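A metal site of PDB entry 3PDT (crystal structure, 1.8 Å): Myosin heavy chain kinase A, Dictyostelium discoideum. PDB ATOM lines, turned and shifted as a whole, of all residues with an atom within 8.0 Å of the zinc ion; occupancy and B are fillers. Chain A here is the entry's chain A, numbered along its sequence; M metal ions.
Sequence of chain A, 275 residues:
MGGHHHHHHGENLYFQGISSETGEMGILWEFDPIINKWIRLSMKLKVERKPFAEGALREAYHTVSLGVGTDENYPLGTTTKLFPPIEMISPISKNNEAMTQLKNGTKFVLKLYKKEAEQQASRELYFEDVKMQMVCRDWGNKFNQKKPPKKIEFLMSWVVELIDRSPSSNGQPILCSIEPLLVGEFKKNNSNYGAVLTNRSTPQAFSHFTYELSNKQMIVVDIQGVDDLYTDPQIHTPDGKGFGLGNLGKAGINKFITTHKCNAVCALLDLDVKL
A ring nitrogen (NE2) of His 208 sits close to the backbone carbonyl oxygen of Asp 272, 3.3 Å away. N of Cys 266 is in hydrogen-bond range of OD1 of Asn 263. O of Cys 266 sits at hydrogen-bond distance from N of Leu 271.
Four residues have an atom within 4 Å of the zinc ion: His 208, His 260, Cys 262 and Cys 266.
The zinc ion is bound by NE2 of His 260 (2.1 Å), ND1 of His 208 (2.1 Å), SG of Cys 266 (2.3 Å) and SG of Cys 262 (2.3 Å).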
ATOM      1  N   SER A 201      10.060  25.421   0.252  1.00  0.00           N
ATOM      2  CA  SER A 201       9.514  24.170   0.814  1.00  0.00           C
ATOM      3  C   SER A 201      10.573  23.174   1.278  1.00  0.00           C
ATOM      4  O   SER A 201      10.480  22.594   2.369  1.00  0.00           O
ATOM      5  CB  SER A 201       8.606  23.466  -0.204  1.00  0.00           C
ATOM      6  OG  SER A 201       7.406  24.173  -0.415  1.00  0.00           O
ATOM      7  N   GLN A 204      12.349  23.203   4.885  1.00  0.00           N
ATOM      8  CA  GLN A 204      11.405  22.914   5.989  1.00  0.00           C
ATOM      9  C   GLN A 204      10.871  21.480   5.942  1.00  0.00           C
ATOM     10  O   GLN A 204      10.669  20.863   6.994  1.00  0.00           O
ATOM     11  CB  GLN A 204      10.237  23.917   6.019  1.00  0.00           C
ATOM     12  CG  GLN A 204      10.634  25.388   5.789  1.00  0.00           C
ATOM     13  CD  GLN A 204      11.695  25.902   6.758  1.00  0.00           C
ATOM     14  OE1 GLN A 204      11.778  25.463   7.908  1.00  0.00           O
ATOM     15  NE2 GLN A 204      12.505  26.840   6.293  1.00  0.00           N
ATOM     16  N   ALA A 205      10.664  20.947   4.747  1.00  0.00           N
ATOM     17  CA  ALA A 205      10.177  19.571   4.603  1.00  0.00           C
ATOM     18  C   ALA A 205      11.244  18.571   5.063  1.00  0.00           C
ATOM     19  O   ALA A 205      10.936  17.567   5.718  1.00  0.00           O
ATOM     20  CB  ALA A 205       9.742  19.295   3.171  1.00  0.00           C
ATOM     21  N   PHE A 206      12.503  18.869   4.757  1.00  0.00           N
ATOM     22  CA  PHE A 206      13.607  18.036   5.247  1.00  0.00           C
ATOM     23  C   PHE A 206      13.672  18.037   6.783  1.00  0.00           C
ATOM     24  O   PHE A 206      13.764  16.970   7.386  1.00  0.00           O
ATOM     25  CB  PHE A 206      14.939  18.489   4.664  1.00  0.00           C
ATOM     26  CG  PHE A 206      16.129  17.807   5.291  1.00  0.00           C
ATOM     27  CD1 PHE A 206      16.426  16.478   4.998  1.00  0.00           C
ATOM     28  CD2 PHE A 206      16.948  18.478   6.177  1.00  0.00           C
ATOM     29  CE1 PHE A 206      17.514  15.831   5.571  1.00  0.00           C
ATOM     30  CE2 PHE A 206      18.040  17.850   6.772  1.00  0.00           C
ATOM     31  CZ  PHE A 206      18.327  16.515   6.461  1.00  0.00           C
ATOM     32  N   SER A 207      13.643  19.210   7.407  1.00  0.00           N
ATOM     33  CA  SER A 207      13.630  19.269   8.872  1.00  0.00           C
ATOM     34  C   SER A 207      12.497  18.378   9.421  1.00  0.00           C
ATOM     35  O   SER A 207      12.716  17.511  10.271  1.00  0.00           O
ATOM     36  CB  SER A 207      13.519  20.713   9.378  1.00  0.00           C
ATOM     37  OG  SER A 207      14.707  21.447   9.143  1.00  0.00           O
ATOM     38  N   HIS A 208      11.285  18.550   8.887  1.00  0.00           N
ATOM     39  CA  HIS A 208      10.157  17.742   9.326  1.00  0.00           C
ATOM     40  C   HIS A 208      10.388  16.236   9.101  1.00  0.00           C
ATOM     41  O   HIS A 208      10.092  15.408   9.967  1.00  0.00           O
ATOM     42  CB  HIS A 208       8.887  18.188   8.592  1.00  0.00           C
ATOM     43  CG  HIS A 208       7.638  17.527   9.084  1.00  0.00           C
ATOM     44  ND1 HIS A 208       6.400  17.824   8.577  1.00  0.00           N
ATOM     45  CD2 HIS A 208       7.437  16.603  10.064  1.00  0.00           C
ATOM     46  CE1 HIS A 208       5.484  17.103   9.206  1.00  0.00           C
ATOM     47  NE2 HIS A 208       6.087  16.358  10.110  1.00  0.00           N
ATOM     48  N   PHE A 209      10.911  15.887   7.923  1.00  0.00           N
ATOM     49  CA  PHE A 209      11.243  14.494   7.577  1.00  0.00           C
ATOM     50  C   PHE A 209      12.150  13.866   8.651  1.00  0.00           C
ATOM     51  O   PHE A 209      11.906  12.745   9.094  1.00  0.00           O
ATOM     52  CB  PHE A 209      11.910  14.443   6.200  1.00  0.00           C
ATOM     53  CG  PHE A 209      12.467  13.089   5.817  1.00  0.00           C
ATOM     54  CD1 PHE A 209      11.667  12.147   5.169  1.00  0.00           C
ATOM     55  CD2 PHE A 209      13.795  12.772   6.095  1.00  0.00           C
ATOM     56  CE1 PHE A 209      12.184  10.902   4.815  1.00  0.00           C
ATOM     57  CE2 PHE A 209      14.312  11.516   5.750  1.00  0.00           C
ATOM     58  CZ  PHE A 209      13.518  10.593   5.102  1.00  0.00           C
ATOM     59  N   GLU A 212      10.117  13.129  11.968  1.00  0.00           N
ATOM     60  CA  GLU A 212       9.201  11.984  11.887  1.00  0.00           C
ATOM     61  C   GLU A 212       9.914  10.640  11.758  1.00  0.00           C
ATOM     62  O   GLU A 212       9.617   9.675  12.489  1.00  0.00           O
ATOM     63  CB  GLU A 212       8.177  12.175  10.757  1.00  0.00           C
ATOM     64  CG  GLU A 212       7.185  11.014  10.670  1.00  0.00           C
ATOM     65  CD  GLU A 212       5.995  11.294   9.776  1.00  0.00           C
ATOM     66  OE1 GLU A 212       5.465  12.416   9.818  1.00  0.00           O
ATOM     67  OE2 GLU A 212       5.595  10.373   9.034  1.00  0.00           O
ATOM     68  N   PHE A 256      10.718  24.619  16.743  1.00  0.00           N
ATOM     69  CA  PHE A 256      10.516  24.243  15.350  1.00  0.00           C
ATOM     70  C   PHE A 256       9.055  23.908  15.071  1.00  0.00           C
ATOM     71  O   PHE A 256       8.483  24.367  14.065  1.00  0.00           O
ATOM     72  CB  PHE A 256      11.383  23.046  14.925  1.00  0.00           C
ATOM     73  CG  PHE A 256      11.106  22.601  13.519  1.00  0.00           C
ATOM     74  CD1 PHE A 256      11.736  23.230  12.448  1.00  0.00           C
ATOM     75  CD2 PHE A 256      10.176  21.587  13.244  1.00  0.00           C
ATOM     76  CE1 PHE A 256      11.459  22.848  11.126  1.00  0.00           C
ATOM     77  CE2 PHE A 256       9.905  21.193  11.918  1.00  0.00           C
ATOM     78  CZ  PHE A 256      10.554  21.826  10.862  1.00  0.00           C
ATOM     79  N   HIS A 260       6.384  25.581  12.223  1.00  0.00           N
ATOM     80  CA  HIS A 260       6.371  24.750  11.002  1.00  0.00           C
ATOM     81  C   HIS A 260       5.002  24.690  10.337  1.00  0.00           C
ATOM     82  O   HIS A 260       4.020  24.287  10.956  1.00  0.00           O
ATOM     83  CB  HIS A 260       6.846  23.308  11.252  1.00  0.00           C
ATOM     84  CG  HIS A 260       6.898  22.475   9.996  1.00  0.00           C
ATOM     85  ND1 HIS A 260       7.720  22.795   8.931  1.00  0.00           N
ATOM     86  CD2 HIS A 260       6.189  21.386   9.607  1.00  0.00           C
ATOM     87  CE1 HIS A 260       7.544  21.913   7.959  1.00  0.00           C
ATOM     88  NE2 HIS A 260       6.636  21.041   8.351  1.00  0.00           N
ATOM     89  N   LYS A 261       4.945  25.088   9.064  1.00  0.00           N
ATOM     90  CA  LYS A 261       3.748  24.885   8.251  1.00  0.00           C
ATOM     91  C   LYS A 261       4.074  23.863   7.180  1.00  0.00           C
ATOM     92  O   LYS A 261       5.028  24.053   6.425  1.00  0.00           O
ATOM     93  CB  LYS A 261       3.298  26.190   7.576  1.00  0.00           C
ATOM     94  CG  LYS A 261       2.972  27.329   8.522  1.00  0.00           C
ATOM     95  CD  LYS A 261       2.684  28.568   7.692  1.00  0.00           C
ATOM     96  CE  LYS A 261       2.539  29.824   8.542  1.00  0.00           C
ATOM     97  NZ  LYS A 261       2.407  30.978   7.609  1.00  0.00           N
ATOM     98  N   CYS A 262       3.306  22.784   7.126  1.00  0.00           N
ATOM     99  CA  CYS A 262       3.569  21.773   6.112  1.00  0.00           C
ATOM    100  C   CYS A 262       3.334  22.338   4.713  1.00  0.00           C
ATOM    101  O   CYS A 262       2.449  23.181   4.518  1.00  0.00           O
ATOM    102  CB  CYS A 262       2.763  20.495   6.349  1.00  0.00           C
ATOM    103  SG  CYS A 262       3.447  19.480   7.694  1.00  0.00           S
ATOM    104  N   ASN A 263       4.148  21.889   3.768  1.00  0.00           N
ATOM    105  CA  ASN A 263       4.135  22.421   2.409  1.00  0.00           C
ATOM    106  C   ASN A 263       3.972  21.292   1.401  1.00  0.00           C
ATOM    107  O   ASN A 263       3.698  20.150   1.788  1.00  0.00           O
ATOM    108  CB  ASN A 263       5.435  23.212   2.151  1.00  0.00           C
ATOM    109  CG  ASN A 263       6.680  22.384   2.405  1.00  0.00           C
ATOM    110  OD1 ASN A 263       6.805  21.273   1.904  1.00  0.00           O
ATOM    111  ND2 ASN A 263       7.597  22.916   3.204  1.00  0.00           N
ATOM    112  N   ALA A 264       4.127  21.597   0.112  1.00  0.00           N
ATOM    113  CA  ALA A 264       3.889  20.610  -0.947  1.00  0.00           C
ATOM    114  C   ALA A 264       4.832  19.410  -0.864  1.00  0.00           C
ATOM    115  O   ALA A 264       4.450  18.303  -1.249  1.00  0.00           O
ATOM    116  CB  ALA A 264       3.966  21.270  -2.334  1.00  0.00           C
ATOM    117  N   VAL A 265       6.050  19.627  -0.337  1.00  0.00           N
ATOM    118  CA  VAL A 265       7.037  18.549  -0.222  1.00  0.00           C
ATOM    119  C   VAL A 265       6.699  17.641   0.962  1.00  0.00           C
ATOM    120  O   VAL A 265       6.736  16.412   0.834  1.00  0.00           O
ATOM    121  CB  VAL A 265       8.501  19.083  -0.177  1.00  0.00           C
ATOM    122  CG1 VAL A 265       9.523  17.940  -0.062  1.00  0.00           C
ATOM    123  CG2 VAL A 265       8.794  19.912  -1.429  1.00  0.00           C
ATOM    124  N   CYS A 266       6.313  18.239   2.099  1.00  0.00           N
ATOM    125  CA  CYS A 266       5.788  17.479   3.232  1.00  0.00           C
ATOM    126  C   CYS A 266       4.682  16.515   2.793  1.00  0.00           C
ATOM    127  O   CYS A 266       4.695  15.348   3.155  1.00  0.00           O
ATOM    128  CB  CYS A 266       5.223  18.403   4.327  1.00  0.00           C
ATOM    129  SG  CYS A 266       6.453  19.484   5.154  1.00  0.00           S
ATOM    130  N   ALA A 267       3.730  17.031   2.001  1.00  0.00           N
ATOM    131  CA  ALA A 267       2.593  16.226   1.551  1.00  0.00           C
ATOM    132  C   ALA A 267       3.035  15.090   0.605  1.00  0.00           C
ATOM    133  O   ALA A 267       2.537  13.971   0.713  1.00  0.00           O
ATOM    134  CB  ALA A 267       1.527  17.108   0.892  1.00  0.00           C
ATOM    135  N   LEU A 271       4.195  13.027   5.133  1.00  0.00           N
ATOM    136  CA  LEU A 271       4.517  13.309   6.534  1.00  0.00           C
ATOM    137  C   LEU A 271       3.238  13.621   7.324  1.00  0.00           C
ATOM    138  O   LEU A 271       2.313  14.223   6.770  1.00  0.00           O
ATOM    139  CB  LEU A 271       5.530  14.452   6.632  1.00  0.00           C
ATOM    140  CG  LEU A 271       6.880  14.243   5.926  1.00  0.00           C
ATOM    141  CD1 LEU A 271       7.825  15.410   6.139  1.00  0.00           C
ATOM    142  CD2 LEU A 271       7.546  12.926   6.367  1.00  0.00           C
ATOM    143  N   ASP A 272       3.208  13.188   8.582  1.00  0.00           N
ATOM    144  CA  ASP A 272       2.097  13.475   9.521  1.00  0.00           C
ATOM    145  C   ASP A 272       1.879  14.977   9.644  1.00  0.00           C
ATOM    146  O   ASP A 272       2.835  15.728   9.844  1.00  0.00           O
ATOM    147  CB  ASP A 272       2.399  12.929  10.930  1.00  0.00           C
ATOM    148  CG  ASP A 272       2.452  11.410  10.995  1.00  0.00           C
ATOM    149  OD1 ASP A 272       1.692  10.729  10.258  1.00  0.00           O
ATOM    150  OD2 ASP A 272       3.256  10.881  11.798  1.00  0.00           O
ATOM    151  N   VAL A 273       0.625  15.406   9.558  1.00  0.00           N
ATOM    152  CA  VAL A 273       0.301  16.828   9.711  1.00  0.00           C
ATOM    153  C   VAL A 273       0.506  17.309  11.159  1.00  0.00           C
ATOM    154  O   VAL A 273       0.778  18.485  11.390  1.00  0.00           O
ATOM    155  CB  VAL A 273      -1.136  17.173   9.231  1.00  0.00           C
ATOM    156  CG1 VAL A 273      -1.260  16.928   7.728  1.00  0.00           C
ATOM    157  CG2 VAL A 273      -2.197  16.385  10.002  1.00  0.00           C
ATOM    158  N   LYS A 274       0.407  16.403  12.124  1.00  0.00           N
ATOM    159  CA  LYS A 274       0.687  16.742  13.515  1.00  0.00           C
ATOM    160  C   LYS A 274       2.069  16.258  13.923  1.00  0.00           C
ATOM    161  O   LYS A 274       2.407  15.074  13.773  1.00  0.00           O
ATOM    162  CB  LYS A 274      -0.378  16.167  14.455  1.00  0.00           C
ATOM    163  CG  LYS A 274      -0.322  16.720  15.871  1.00  0.00           C
ATOM    164  CD  LYS A 274      -0.908  18.137  15.972  1.00  0.00           C
ATOM    165  CE  LYS A 274      -0.858  18.660  17.397  1.00  0.00           C
ATOM    166  NZ  LYS A 274      -1.636  17.817  18.346  1.00  0.00           N
ATOM    167  N   LEU A 275       2.882  17.175  14.434  1.00  0.00           N
ATOM    168  CA  LEU A 275       4.241  16.857  14.893  1.00  0.00           C
ATOM    169  C   LEU A 275       4.254  16.632  16.409  1.00  0.00           C
ATOM    170  O   LEU A 275       3.512  17.278  17.148  1.00  0.00           O
ATOM    171  CB  LEU A 275       5.221  17.969  14.505  1.00  0.00           C
ATOM    172  CG  LEU A 275       5.619  18.106  13.039  1.00  0.00           C
ATOM    173  CD1 LEU A 275       4.470  18.573  12.143  1.00  0.00           C
ATOM    174  CD2 LEU A 275       6.814  19.050  12.893  1.00  0.00           C
HETATM  175 ZN    ZN M   1       5.742  19.423   7.329  1.00  0.00          ZN
